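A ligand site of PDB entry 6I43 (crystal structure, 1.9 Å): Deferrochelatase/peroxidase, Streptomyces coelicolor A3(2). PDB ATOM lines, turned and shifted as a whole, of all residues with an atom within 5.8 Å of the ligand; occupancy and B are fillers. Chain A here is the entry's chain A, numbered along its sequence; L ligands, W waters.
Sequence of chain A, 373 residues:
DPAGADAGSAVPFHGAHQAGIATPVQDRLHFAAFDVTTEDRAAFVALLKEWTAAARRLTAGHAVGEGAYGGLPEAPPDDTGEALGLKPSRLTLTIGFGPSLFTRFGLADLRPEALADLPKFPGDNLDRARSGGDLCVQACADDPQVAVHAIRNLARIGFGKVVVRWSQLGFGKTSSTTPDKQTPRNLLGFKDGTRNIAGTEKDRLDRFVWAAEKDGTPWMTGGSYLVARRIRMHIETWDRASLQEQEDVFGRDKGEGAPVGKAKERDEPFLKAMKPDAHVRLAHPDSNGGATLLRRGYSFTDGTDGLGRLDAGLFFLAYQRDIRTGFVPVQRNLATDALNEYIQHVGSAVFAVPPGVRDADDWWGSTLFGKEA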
ATOM      1  N   ASN A 186      13.014  30.011 -14.372  1.00  0.00           N
ATOM      2  CA  ASN A 186      12.405  28.873 -15.048  1.00  0.00           C
ATOM      3  C   ASN A 186      11.867  29.313 -16.414  1.00  0.00           C
ATOM      4  O   ASN A 186      11.978  30.479 -16.821  1.00  0.00           O
ATOM      5  CB  ASN A 186      11.317  28.261 -14.175  1.00  0.00           C
ATOM      6  CG  ASN A 186      10.254  29.245 -13.794  1.00  0.00           C
ATOM      7  OD1 ASN A 186       9.747  29.989 -14.637  1.00  0.00           O
ATOM      8  ND2 ASN A 186       9.930  29.287 -12.501  1.00  0.00           N
ATOM      9  N   LEU A 188       8.923  29.736 -17.480  1.00  0.00           N
ATOM     10  CA  LEU A 188       7.856  30.734 -17.447  1.00  0.00           C
ATOM     11  C   LEU A 188       8.390  32.149 -17.288  1.00  0.00           C
ATOM     12  O   LEU A 188       7.598  33.103 -17.337  1.00  0.00           O
ATOM     13  CB  LEU A 188       6.894  30.404 -16.302  1.00  0.00           C
ATOM     14  CG  LEU A 188       6.257  29.011 -16.354  1.00  0.00           C
ATOM     15  CD1 LEU A 188       5.191  28.880 -15.289  1.00  0.00           C
ATOM     16  CD2 LEU A 188       5.663  28.728 -17.713  1.00  0.00           C
ATOM     17  N   PHE A 190      10.059  33.458 -14.668  1.00  0.00           N
ATOM     18  CA  PHE A 190      10.134  33.962 -13.300  1.00  0.00           C
ATOM     19  C   PHE A 190      11.355  33.411 -12.575  1.00  0.00           C
ATOM     20  O   PHE A 190      11.747  32.260 -12.785  1.00  0.00           O
ATOM     21  CB  PHE A 190       8.867  33.606 -12.513  1.00  0.00           C
ATOM     22  CG  PHE A 190       7.732  34.534 -12.769  1.00  0.00           C
ATOM     23  CD1 PHE A 190       6.982  34.442 -13.948  1.00  0.00           C
ATOM     24  CD2 PHE A 190       7.386  35.501 -11.832  1.00  0.00           C
ATOM     25  CE1 PHE A 190       5.942  35.302 -14.188  1.00  0.00           C
ATOM     26  CE2 PHE A 190       6.321  36.367 -12.086  1.00  0.00           C
ATOM     27  CZ  PHE A 190       5.621  36.276 -13.272  1.00  0.00           C
ATOM     28  N   LYS A 191      11.973  34.244 -11.739  1.00  0.00           N
ATOM     29  CA  LYS A 191      13.012  33.766 -10.827  1.00  0.00           C
ATOM     30  C   LYS A 191      12.436  32.680  -9.942  1.00  0.00           C
ATOM     31  O   LYS A 191      11.309  32.770  -9.466  1.00  0.00           O
ATOM     32  CB  LYS A 191      13.535  34.902  -9.960  1.00  0.00           C
ATOM     33  CG  LYS A 191      14.227  35.969 -10.732  1.00  0.00           C
ATOM     34  CD  LYS A 191      14.640  37.121  -9.763  1.00  0.00           C
ATOM     35  CE  LYS A 191      15.493  38.177 -10.451  1.00  0.00           C
ATOM     36  NZ  LYS A 191      15.824  39.313  -9.518  1.00  0.00           N
ATOM     37  N   ASP A 192      13.219  31.644  -9.729  1.00  0.00           N
ATOM     38  CA  ASP A 192      12.751  30.460  -9.027  1.00  0.00           C
ATOM     39  C   ASP A 192      13.868  30.066  -8.072  1.00  0.00           C
ATOM     40  O   ASP A 192      14.943  29.669  -8.526  1.00  0.00           O
ATOM     41  CB  ASP A 192      12.431  29.335 -10.025  1.00  0.00           C
ATOM     42  CG  ASP A 192      11.447  28.316  -9.471  1.00  0.00           C
ATOM     43  OD1 ASP A 192      11.272  28.224  -8.233  1.00  0.00           O
ATOM     44  OD2 ASP A 192      10.822  27.616 -10.294  1.00  0.00           O
ATOM     45  N   GLY A 193      13.622  30.205  -6.771  1.00  0.00           N
ATOM     46  CA  GLY A 193      14.610  29.874  -5.764  1.00  0.00           C
ATOM     47  C   GLY A 193      14.910  30.955  -4.729  1.00  0.00           C
ATOM     48  O   GLY A 193      15.755  30.760  -3.854  1.00  0.00           O
ATOM     49  N   THR A 194      14.182  32.075  -4.791  1.00  0.00           N
ATOM     50  CA  THR A 194      14.449  33.204  -3.908  1.00  0.00           C
ATOM     51  C   THR A 194      14.360  32.804  -2.445  1.00  0.00           C
ATOM     52  O   THR A 194      15.316  33.008  -1.674  1.00  0.00           O
ATOM     53  CB  THR A 194      13.480  34.344  -4.201  1.00  0.00           C
ATOM     54  OG1 THR A 194      13.642  34.744  -5.557  1.00  0.00           O
ATOM     55  CG2 THR A 194      13.753  35.575  -3.283  1.00  0.00           C
ATOM     56  N   ARG A 195      13.227  32.258  -2.025  1.00  0.00           N
ATOM     57  CA  ARG A 195      12.994  31.864  -0.625  1.00  0.00           C
ATOM     58  C   ARG A 195      13.114  30.346  -0.524  1.00  0.00           C
ATOM     59  O   ARG A 195      12.128  29.622  -0.445  1.00  0.00           O
ATOM     60  CB  ARG A 195      11.641  32.377  -0.129  1.00  0.00           C
ATOM     61  CG  ARG A 195      11.702  33.855   0.300  1.00  0.00           C
ATOM     62  CD  ARG A 195      10.380  34.414   0.920  1.00  0.00           C
ATOM     63  NE  ARG A 195       9.735  33.342   1.640  1.00  0.00           N
ATOM     64  CZ  ARG A 195      10.081  32.940   2.850  1.00  0.00           C
ATOM     65  NH1 ARG A 195       9.505  31.874   3.375  1.00  0.00           N
ATOM     66  NH2 ARG A 195      10.994  33.636   3.548  1.00  0.00           N
ATOM     67  N   ASN A 196      14.351  29.867  -0.516  1.00  0.00           N
ATOM     68  CA  ASN A 196      14.665  28.454  -0.346  1.00  0.00           C
ATOM     69  C   ASN A 196      15.402  28.320   0.991  1.00  0.00           C
ATOM     70  O   ASN A 196      15.241  29.158   1.879  1.00  0.00           O
ATOM     71  CB  ASN A 196      15.458  27.957  -1.557  1.00  0.00           C
ATOM     72  CG  ASN A 196      15.420  26.458  -1.732  1.00  0.00           C
ATOM     73  OD1 ASN A 196      14.461  25.802  -1.348  1.00  0.00           O
ATOM     74  ND2 ASN A 196      16.474  25.910  -2.342  1.00  0.00           N
ATOM     75  N   ILE A 231       7.156  17.855 -14.268  1.00  0.00           N
ATOM     76  CA  ILE A 231       6.027  18.769 -14.455  1.00  0.00           C
ATOM     77  C   ILE A 231       6.087  19.354 -15.855  1.00  0.00           C
ATOM     78  O   ILE A 231       7.024  20.075 -16.207  1.00  0.00           O
ATOM     79  CB  ILE A 231       6.005  19.874 -13.396  1.00  0.00           C
ATOM     80  CG1 ILE A 231       5.907  19.263 -11.997  1.00  0.00           C
ATOM     81  CG2 ILE A 231       4.797  20.793 -13.607  1.00  0.00           C
ATOM     82  CD1 ILE A 231       6.125  20.249 -10.888  1.00  0.00           C
ATOM     83  N   MET A 233       4.831  21.988 -18.643  1.00  0.00           N
ATOM     84  CA  MET A 233       4.333  23.364 -18.656  1.00  0.00           C
ATOM     85  C   MET A 233       3.562  23.589 -19.936  1.00  0.00           C
ATOM     86  O   MET A 233       4.021  23.210 -21.015  1.00  0.00           O
ATOM     87  CB  MET A 233       5.478  24.379 -18.578  1.00  0.00           C
ATOM     88  CG  MET A 233       6.105  24.471 -17.202  1.00  0.00           C
ATOM     89  SD  MET A 233       7.687  25.318 -17.327  1.00  0.00           S
ATOM     90  CE  MET A 233       8.007  25.651 -15.619  1.00  0.00           C
ATOM     91  N   PHE A 250       1.669  34.166  -9.503  1.00  0.00           N
ATOM     92  CA  PHE A 250       2.720  33.913  -8.527  1.00  0.00           C
ATOM     93  C   PHE A 250       2.649  34.802  -7.277  1.00  0.00           C
ATOM     94  O   PHE A 250       2.934  34.325  -6.182  1.00  0.00           O
ATOM     95  CB  PHE A 250       4.107  34.066  -9.156  1.00  0.00           C
ATOM     96  CG  PHE A 250       4.448  32.919 -10.058  1.00  0.00           C
ATOM     97  CD1 PHE A 250       4.640  31.648  -9.540  1.00  0.00           C
ATOM     98  CD2 PHE A 250       4.529  33.105 -11.423  1.00  0.00           C
ATOM     99  CE1 PHE A 250       4.918  30.570 -10.381  1.00  0.00           C
ATOM    100  CE2 PHE A 250       4.807  32.027 -12.264  1.00  0.00           C
ATOM    101  CZ  PHE A 250       5.000  30.764 -11.717  1.00  0.00           C
ATOM    102  N   ARG A 252       4.497  37.678  -7.292  1.00  0.00           N
ATOM    103  CA  ARG A 252       5.724  38.441  -7.425  1.00  0.00           C
ATOM    104  C   ARG A 252       5.721  39.042  -8.823  1.00  0.00           C
ATOM    105  O   ARG A 252       5.081  38.519  -9.729  1.00  0.00           O
ATOM    106  CB  ARG A 252       6.973  37.569  -7.259  1.00  0.00           C
ATOM    107  CG  ARG A 252       7.239  37.090  -5.841  1.00  0.00           C
ATOM    108  CD  ARG A 252       8.429  36.165  -5.796  1.00  0.00           C
ATOM    109  NE  ARG A 252       8.713  35.710  -4.427  1.00  0.00           N
ATOM    110  CZ  ARG A 252       9.517  36.343  -3.559  1.00  0.00           C
ATOM    111  NH1 ARG A 252      10.161  37.454  -3.906  1.00  0.00           N
ATOM    112  NH2 ARG A 252       9.704  35.843  -2.352  1.00  0.00           N
ATOM    113  N   PRO A 269       7.781  38.669   1.546  1.00  0.00           N
ATOM    114  CA  PRO A 269       6.414  38.744   1.016  1.00  0.00           C
ATOM    115  C   PRO A 269       5.444  39.203   2.098  1.00  0.00           C
ATOM    116  O   PRO A 269       5.582  38.868   3.277  1.00  0.00           O
ATOM    117  CB  PRO A 269       6.133  37.315   0.535  1.00  0.00           C
ATOM    118  CG  PRO A 269       7.134  36.466   1.146  1.00  0.00           C
ATOM    119  CD  PRO A 269       8.344  37.316   1.429  1.00  0.00           C
ATOM    120  N   HIS A 279       0.526  31.426  -6.084  1.00  0.00           N
ATOM    121  CA  HIS A 279       1.396  30.305  -5.785  1.00  0.00           C
ATOM    122  C   HIS A 279       2.233  30.544  -4.527  1.00  0.00           C
ATOM    123  O   HIS A 279       2.342  29.669  -3.663  1.00  0.00           O
ATOM    124  CB  HIS A 279       2.289  30.059  -6.995  1.00  0.00           C
ATOM    125  CG  HIS A 279       3.254  28.940  -6.817  1.00  0.00           C
ATOM    126  ND1 HIS A 279       2.857  27.624  -6.847  1.00  0.00           N
ATOM    127  CD2 HIS A 279       4.589  28.937  -6.609  1.00  0.00           C
ATOM    128  CE1 HIS A 279       3.904  26.849  -6.655  1.00  0.00           C
ATOM    129  NE2 HIS A 279       4.969  27.623  -6.516  1.00  0.00           N
ATOM    130  N   VAL A 280       2.878  31.710  -4.443  1.00  0.00           N
ATOM    131  CA  VAL A 280       3.724  32.003  -3.297  1.00  0.00           C
ATOM    132  C   VAL A 280       2.884  32.002  -2.032  1.00  0.00           C
ATOM    133  O   VAL A 280       3.282  31.436  -0.999  1.00  0.00           O
ATOM    134  CB  VAL A 280       4.458  33.328  -3.509  1.00  0.00           C
ATOM    135  CG1 VAL A 280       5.132  33.793  -2.223  1.00  0.00           C
ATOM    136  CG2 VAL A 280       5.494  33.188  -4.584  1.00  0.00           C
ATOM    137  N   ALA A 283       2.122  28.380  -1.096  1.00  0.00           N
ATOM    138  CA  ALA A 283       3.285  27.532  -0.849  1.00  0.00           C
ATOM    139  C   ALA A 283       4.119  27.990   0.340  1.00  0.00           C
ATOM    140  O   ALA A 283       4.930  27.210   0.819  1.00  0.00           O
ATOM    141  CB  ALA A 283       4.190  27.495  -2.094  1.00  0.00           C
ATOM    142  N   HIS A 284       3.905  29.225   0.802  1.00  0.00           N
ATOM    143  CA  HIS A 284       4.720  29.824   1.855  1.00  0.00           C
ATOM    144  C   HIS A 284       4.607  29.038   3.156  1.00  0.00           C
ATOM    145  O   HIS A 284       3.550  28.492   3.478  1.00  0.00           O
ATOM    146  CB  HIS A 284       4.260  31.269   2.071  1.00  0.00           C
ATOM    147  CG  HIS A 284       5.189  32.103   2.907  1.00  0.00           C
ATOM    148  ND1 HIS A 284       5.260  31.987   4.277  1.00  0.00           N
ATOM    149  CD2 HIS A 284       6.075  33.064   2.564  1.00  0.00           C
ATOM    150  CE1 HIS A 284       6.157  32.849   4.746  1.00  0.00           C
ATOM    151  NE2 HIS A 284       6.664  33.511   3.720  1.00  0.00           N
ATOM    152  N   PRO A 285       5.693  28.939   3.931  1.00  0.00           N
ATOM    153  CA  PRO A 285       5.634  28.145   5.172  1.00  0.00           C
ATOM    154  C   PRO A 285       4.541  28.610   6.106  1.00  0.00           C
ATOM    155  O   PRO A 285       3.890  27.785   6.747  1.00  0.00           O
ATOM    156  CB  PRO A 285       7.040  28.324   5.757  1.00  0.00           C
ATOM    157  CG  PRO A 285       7.901  28.520   4.618  1.00  0.00           C
ATOM    158  CD  PRO A 285       7.071  29.322   3.624  1.00  0.00           C
ATOM    159  N   LEU A 293      10.724  23.493   2.573  1.00  0.00           N
ATOM    160  CA  LEU A 293      11.348  22.529   1.677  1.00  0.00           C
ATOM    161  C   LEU A 293      12.676  23.059   1.186  1.00  0.00           C
ATOM    162  O   LEU A 293      12.876  24.269   1.112  1.00  0.00           O
ATOM    163  CB  LEU A 293      10.459  22.296   0.438  1.00  0.00           C
ATOM    164  CG  LEU A 293       9.034  21.872   0.692  1.00  0.00           C
ATOM    165  CD1 LEU A 293       8.277  21.793  -0.633  1.00  0.00           C
ATOM    166  CD2 LEU A 293       9.035  20.530   1.357  1.00  0.00           C
ATOM    167  N   ARG A 295      14.185  23.104  -2.265  1.00  0.00           N
ATOM    168  CA  ARG A 295      13.933  22.900  -3.672  1.00  0.00           C
ATOM    169  C   ARG A 295      15.229  22.934  -4.465  1.00  0.00           C
ATOM    170  O   ARG A 295      16.074  23.818  -4.251  1.00  0.00           O
ATOM    171  CB  ARG A 295      12.968  23.967  -4.204  1.00  0.00           C
ATOM    172  CG  ARG A 295      11.603  23.911  -3.536  1.00  0.00           C
ATOM    173  CD  ARG A 295      10.758  25.052  -3.950  1.00  0.00           C
ATOM    174  NE  ARG A 295      11.197  26.277  -3.315  1.00  0.00           N
ATOM    175  CZ  ARG A 295      11.270  27.471  -3.903  1.00  0.00           C
ATOM    176  NH1 ARG A 295      10.924  27.637  -5.179  1.00  0.00           N
ATOM    177  NH2 ARG A 295      11.687  28.499  -3.174  1.00  0.00           N
ATOM    178  N   LEU A 314       9.548  21.374 -16.006  1.00  0.00           N
ATOM    179  CA  LEU A 314      10.381  21.591 -14.835  1.00  0.00           C
ATOM    180  C   LEU A 314      10.465  20.258 -14.129  1.00  0.00           C
ATOM    181  O   LEU A 314       9.441  19.622 -13.864  1.00  0.00           O
ATOM    182  CB  LEU A 314       9.793  22.685 -13.955  1.00  0.00           C
ATOM    183  CG  LEU A 314      10.722  23.260 -12.922  1.00  0.00           C
ATOM    184  CD1 LEU A 314      10.360  24.698 -12.603  1.00  0.00           C
ATOM    185  CD2 LEU A 314      10.681  22.390 -11.655  1.00  0.00           C
ATOM    186  N   PHE A 316      10.996  18.953 -10.912  1.00  0.00           N
ATOM    187  CA  PHE A 316      10.951  19.480  -9.558  1.00  0.00           C
ATOM    188  C   PHE A 316      11.574  18.483  -8.592  1.00  0.00           C
ATOM    189  O   PHE A 316      11.215  17.312  -8.578  1.00  0.00           O
ATOM    190  CB  PHE A 316       9.483  19.765  -9.189  1.00  0.00           C
ATOM    191  CG  PHE A 316       9.297  20.358  -7.810  1.00  0.00           C
ATOM    192  CD1 PHE A 316       9.409  21.715  -7.604  1.00  0.00           C
ATOM    193  CD2 PHE A 316       9.001  19.548  -6.725  1.00  0.00           C
ATOM    194  CE1 PHE A 316       9.237  22.258  -6.344  1.00  0.00           C
ATOM    195  CE2 PHE A 316       8.826  20.078  -5.465  1.00  0.00           C
ATOM    196  CZ  PHE A 316       8.942  21.440  -5.271  1.00  0.00           C
ATOM    197  N   PHE A 327       6.758  17.937   1.591  1.00  0.00           N
ATOM    198  CA  PHE A 327       6.091  18.047   0.292  1.00  0.00           C
ATOM    199  C   PHE A 327       4.585  17.853   0.406  1.00  0.00           C
ATOM    200  O   PHE A 327       3.809  18.606  -0.205  1.00  0.00           O
ATOM    201  CB  PHE A 327       6.689  17.036  -0.677  1.00  0.00           C
ATOM    202  CG  PHE A 327       6.055  17.034  -2.028  1.00  0.00           C
ATOM    203  CD1 PHE A 327       6.444  17.962  -2.990  1.00  0.00           C
ATOM    204  CD2 PHE A 327       5.050  16.131  -2.332  1.00  0.00           C
ATOM    205  CE1 PHE A 327       5.842  17.976  -4.223  1.00  0.00           C
ATOM    206  CE2 PHE A 327       4.462  16.142  -3.578  1.00  0.00           C
ATOM    207  CZ  PHE A 327       4.854  17.061  -4.535  1.00  0.00           C
ATOM    208  N   VAL A 330       2.430  20.898   1.653  1.00  0.00           N
ATOM    209  CA  VAL A 330       2.529  22.004   0.717  1.00  0.00           C
ATOM    210  C   VAL A 330       1.777  21.683  -0.575  1.00  0.00           C
ATOM    211  O   VAL A 330       0.965  22.471  -1.041  1.00  0.00           O
ATOM    212  CB  VAL A 330       4.003  22.364   0.475  1.00  0.00           C
ATOM    213  CG1 VAL A 330       4.107  23.495  -0.537  1.00  0.00           C
ATOM    214  CG2 VAL A 330       4.687  22.754   1.793  1.00  0.00           C
ATOM    215  N   GLN A 331       2.026  20.509  -1.151  1.00  0.00           N
ATOM    216  CA  GLN A 331       1.338  20.187  -2.404  1.00  0.00           C
ATOM    217  C   GLN A 331      -0.166  20.067  -2.220  1.00  0.00           C
ATOM    218  O   GLN A 331      -0.932  20.387  -3.138  1.00  0.00           O
ATOM    219  CB  GLN A 331       1.908  18.894  -2.993  1.00  0.00           C
ATOM    220  CG  GLN A 331       1.238  18.435  -4.291  1.00  0.00           C
ATOM    221  CD  GLN A 331       1.418  19.374  -5.477  1.00  0.00           C
ATOM    222  OE1 GLN A 331       2.438  20.050  -5.624  1.00  0.00           O
ATOM    223  NE2 GLN A 331       0.438  19.392  -6.353  1.00  0.00           N
ATOM    224  N   LEU A 334      -1.607  23.327  -2.599  1.00  0.00           N
ATOM    225  CA  LEU A 334      -1.624  23.867  -3.949  1.00  0.00           C
ATOM    226  C   LEU A 334      -2.807  23.369  -4.768  1.00  0.00           C
ATOM    227  O   LEU A 334      -2.850  23.613  -5.983  1.00  0.00           O
ATOM    228  CB  LEU A 334      -0.321  23.522  -4.653  1.00  0.00           C
ATOM    229  CG  LEU A 334       0.967  24.026  -3.992  1.00  0.00           C
ATOM    230  CD1 LEU A 334       2.155  23.705  -4.914  1.00  0.00           C
ATOM    231  CD2 LEU A 334       0.887  25.529  -3.691  1.00  0.00           C
ATOM    232  N   LEU A 339      -1.478  28.493 -10.520  1.00  0.00           N
ATOM    233  CA  LEU A 339      -0.508  27.900 -11.428  1.00  0.00           C
ATOM    234  C   LEU A 339      -1.022  26.607 -12.048  1.00  0.00           C
ATOM    235  O   LEU A 339      -0.545  26.202 -13.101  1.00  0.00           O
ATOM    236  CB  LEU A 339       0.802  27.655 -10.671  1.00  0.00           C
ATOM    237  CG  LEU A 339       2.007  27.121 -11.451  1.00  0.00           C
ATOM    238  CD1 LEU A 339       2.442  28.092 -12.541  1.00  0.00           C
ATOM    239  CD2 LEU A 339       3.126  26.858 -10.490  1.00  0.00           C
ATOM    240  N   ILE A 343       0.254  23.939 -15.682  1.00  0.00           N
ATOM    241  CA  ILE A 343       1.202  22.847 -15.456  1.00  0.00           C
ATOM    242  C   ILE A 343       0.423  21.538 -15.326  1.00  0.00           C
ATOM    243  O   ILE A 343      -0.782  21.532 -15.098  1.00  0.00           O
ATOM    244  CB  ILE A 343       2.065  23.072 -14.197  1.00  0.00           C
ATOM    245  CG1 ILE A 343       1.208  23.062 -12.918  1.00  0.00           C
ATOM    246  CG2 ILE A 343       2.813  24.397 -14.305  1.00  0.00           C
ATOM    247  CD1 ILE A 343       1.986  23.090 -11.660  1.00  0.00           C
ATOM    248  N   HIS A 345       1.512  17.579 -13.540  1.00  0.00           N
ATOM    249  CA  HIS A 345       2.444  16.600 -13.009  1.00  0.00           C
ATOM    250  C   HIS A 345       2.281  15.301 -13.789  1.00  0.00           C
ATOM    251  O   HIS A 345       1.180  14.728 -13.817  1.00  0.00           O
ATOM    252  CB  HIS A 345       2.218  16.352 -11.527  1.00  0.00           C
ATOM    253  CG  HIS A 345       2.464  17.544 -10.670  1.00  0.00           C
ATOM    254  ND1 HIS A 345       3.362  17.530  -9.614  1.00  0.00           N
ATOM    255  CD2 HIS A 345       1.922  18.786 -10.690  1.00  0.00           C
ATOM    256  CE1 HIS A 345       3.367  18.718  -9.041  1.00  0.00           C
ATOM    257  NE2 HIS A 345       2.503  19.495  -9.664  1.00  0.00           N
HETATM  258  C1  LIG L   1       8.106  29.612  -4.834  1.00  0.00           C
HETATM  259  C2  LIG L   1       7.537  28.698  -9.541  1.00  0.00           C
HETATM  260  C3  LIG L   1       6.183  24.195  -8.449  1.00  0.00           C
HETATM  261  C4  LIG L   1       6.903  25.099  -3.744  1.00  0.00           C
HETATM  262  C5  LIG L   1       8.042  29.762  -6.192  1.00  0.00           C
HETATM  263  C6  LIG L   1       8.364  30.991  -6.899  1.00  0.00           C
HETATM  264  C7  LIG L   1       8.197  30.717  -8.195  1.00  0.00           C
HETATM  265  C8  LIG L   1       7.778  29.345  -8.350  1.00  0.00           C
HETATM  266  C9  LIG L   1       8.356  31.676  -9.395  1.00  0.00           C
HETATM  267  C10 LIG L   1       8.753  32.353  -6.239  1.00  0.00           C
HETATM  268  C11 LIG L   1      10.266  32.526  -6.000  1.00  0.00           C
HETATM  269  C12 LIG L   1      10.821  31.583  -4.972  1.00  0.00           C
HETATM  270  O1  LIG L   1      11.364  30.521  -5.375  1.00  0.00           O
HETATM  271  O2  LIG L   1      10.742  31.882  -3.749  1.00  0.00           O
HETATM  272  C13 LIG L   1       7.132  27.397  -9.657  1.00  0.00           C
HETATM  273  C14 LIG L   1       6.868  26.696 -10.915  1.00  0.00           C
HETATM  274  C15 LIG L   1       6.479  25.445 -10.613  1.00  0.00           C
HETATM  275  C16 LIG L   1       6.511  25.320  -9.163  1.00  0.00           C
HETATM  276  C17 LIG L   1       7.015  27.406 -12.290  1.00  0.00           C
HETATM  277  C18 LIG L   1       6.103  24.263 -11.535  1.00  0.00           C
HETATM  278  C19 LIG L   1       6.376  24.190 -12.827  1.00  0.00           C
HETATM  279  C20 LIG L   1       6.236  24.062  -7.078  1.00  0.00           C
HETATM  280  C21 LIG L   1       5.862  22.877  -6.335  1.00  0.00           C
HETATM  281  C22 LIG L   1       6.077  23.131  -5.057  1.00  0.00           C
HETATM  282  C23 LIG L   1       6.572  24.482  -4.934  1.00  0.00           C
HETATM  283  C24 LIG L   1       5.367  21.578  -6.992  1.00  0.00           C
HETATM  284  C25 LIG L   1       5.836  22.275  -3.810  1.00  0.00           C
HETATM  285  C26 LIG L   1       4.914  21.331  -3.718  1.00  0.00           C
HETATM  286  C27 LIG L   1       7.342  26.392  -3.603  1.00  0.00           C
HETATM  287  C28 LIG L   1       7.803  27.034  -2.388  1.00  0.00           C
HETATM  288  C29 LIG L   1       8.111  28.305  -2.691  1.00  0.00           C
HETATM  289  C30 LIG L   1       7.888  28.466  -4.117  1.00  0.00           C
HETATM  290  C31 LIG L   1       7.822  26.370  -0.999  1.00  0.00           C
HETATM  291  C32 LIG L   1       8.629  29.416  -1.747  1.00  0.00           C
HETATM  292  C33 LIG L   1       7.462  30.134  -1.070  1.00  0.00           C
HETATM  293  C34 LIG L   1       7.974  31.059   0.013  1.00  0.00           C
HETATM  294  O3  LIG L   1       7.997  32.274  -0.219  1.00  0.00           O
HETATM  295  O4  LIG L   1       8.374  30.589   1.094  1.00  0.00           O
HETATM  296  N1  LIG L   1       7.698  28.783  -7.111  1.00  0.00           N
HETATM  297  N2  LIG L   1       6.913  26.522  -8.635  1.00  0.00           N
HETATM  298  N3  LIG L   1       6.645  25.039  -6.179  1.00  0.00           N
HETATM  299  N4  LIG L   1       7.466  27.283  -4.642  1.00  0.00           N
HETATM  300 FE1  LIG L   1       7.055  26.959  -6.641  1.00  0.00          FE
HETATM  301  O   HOH W   1       2.087  21.673  -7.988  1.00  0.00           O
HETATM  302  O   HOH W   2      10.311  28.794   1.503  1.00  0.00           O
HETATM  303  O   HOH W   3       9.960  25.325  -9.427  1.00  0.00           O
HETATM  304  O   HOH W   4       6.997  25.718   2.122  1.00  0.00           O
HETATM  305  O   HOH W   5       9.357  26.380  -7.038  1.00  0.00           O
HETATM  306  O   HOH W   6       9.687  26.117   1.637  1.00  0.00           O
HETATM  307  O   HOH W   7       8.663  33.370  -2.734  1.00  0.00           O
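An iron atom (FE1) of the ligand is bound by a ring nitrogen (NE2) of His 279 (2.2 Å). The backbone NH (N) of Gly 193 sits at hydrogen-bond distance from an oxygen (O1) of the ligand, 2.7 Å away. The backbone NH (N) of Arg 195 is in hydrogen-bond range of an oxygen (O2) of the ligand (3.0 Å). The backbone NH of Thr 194 is in hydrogen-bond range of an oxygen (O1) of the ligand, 3.3 Å away. The guanidinium group (NE) of Arg 195 lies within salt-bridge range of an oxygen (O3) of the ligand (2.8 Å). The guanidinium group of Arg 295 is in salt-bridge range of an oxygen (O1) of the ligand (2.9 Å).
The guanidinium group (NH1) of Arg 195 is in hydrogen-bond range of a ring nitrogen (NE2) of His 284 (3.3 Å). The side-chain amide oxygen of Asn 186 is in hydrogen-bond range of the backbone NH of Phe 190 (3.5 Å). The backbone carbonyl oxygen (O) of Arg 195 lies within hydrogen-bond range of the guanidinium group (NH2) of Arg 295. The side-chain carboxylate (OD2) of Asp 192 sits at hydrogen-bond distance from the side-chain amide nitrogen (ND2) of Asn 186, 2.9 Å away. The backbone NH (N) of Val 280 lies within hydrogen-bond range of the backbone carbonyl oxygen (O) of Phe 250 (3.1 Å). OD1 of Asn 186 is in hydrogen-bond range of N of Leu 188, 3.0 Å away. The side-chain carboxylate (OD1) of Asp 192 is in salt-bridge range of the guanidinium group (NH1) of Arg 295 (3.1 Å). The backbone carbonyl oxygen (O) of Ile 231 sits at hydrogen-bond distance from the backbone NH (N) of Leu 314.
Merely in contact with the ligand: Asn 186 (3.5 Å), Leu 188 (3.8 Å), Phe 190 (3.7 Å), Lys 191 (3.1 Å), Asp 192 (3.5 Å), Ile 231 (3.8 Å), Met 233 (3.5 Å), Phe 250 (3.3 Å), Arg 252 (3.8 Å), Val 280 (3.7 Å), Ala 283 (3.5 Å), His 284 (3.5 Å), Pro 285 (3.1 Å), Leu 314 (3.9 Å), Phe 316 (3.3 Å), Phe 327 (3.5 Å), Val 330 (3.9 Å), Gln 331 (3.4 Å), Leu 334 (3.8 Å), Leu 339 (3.6 Å) and Ile 343 (3.9 Å). Hydrophobic or aromatic side chains that line the ligand: Leu 188, Phe 190, Ile 231, Met 233, Phe 250, His 279, Val 280, Ala 283, His 284, Pro 285, Leu 314, Phe 316, Phe 327, Val 330, Leu 334, Leu 339 and Ile 343. Within 4 Å of the ligand: Asn 186, Leu 188, Phe 190, Lys 191, Asp 192, Gly 193, Thr 194, Arg 195, Ile 231, Met 233, Phe 250, Arg 252, His 279, Val 280, Ala 283, His 284, Pro 285, Arg 295, Leu 314, Phe 316, Phe 327, Val 330, Gln 331, Leu 334, Leu 339 and Ile 343. The nearest printed residue that does not touch the ligand is Leu 293 (4.04 Å).
Water W5 lies within hydrogen-bond range of NH1 of Arg 295 (2.7 Å) and OD1 of Asp 192 (2.9 Å). Water W2 lies within hydrogen-bond range of O4 of the ligand (2.7 Å) and O of Arg 195 (2.8 Å). Water W7 bridges the guanidinium group of Arg 252 (2.7 Å) and an oxygen (O2) of the ligand (2.8 Å). Water W1 bridges a ring nitrogen (NE2) of His 345 (2.8 Å) and the side-chain amide oxygen (OE1) of Gln 331 (2.9 Å).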
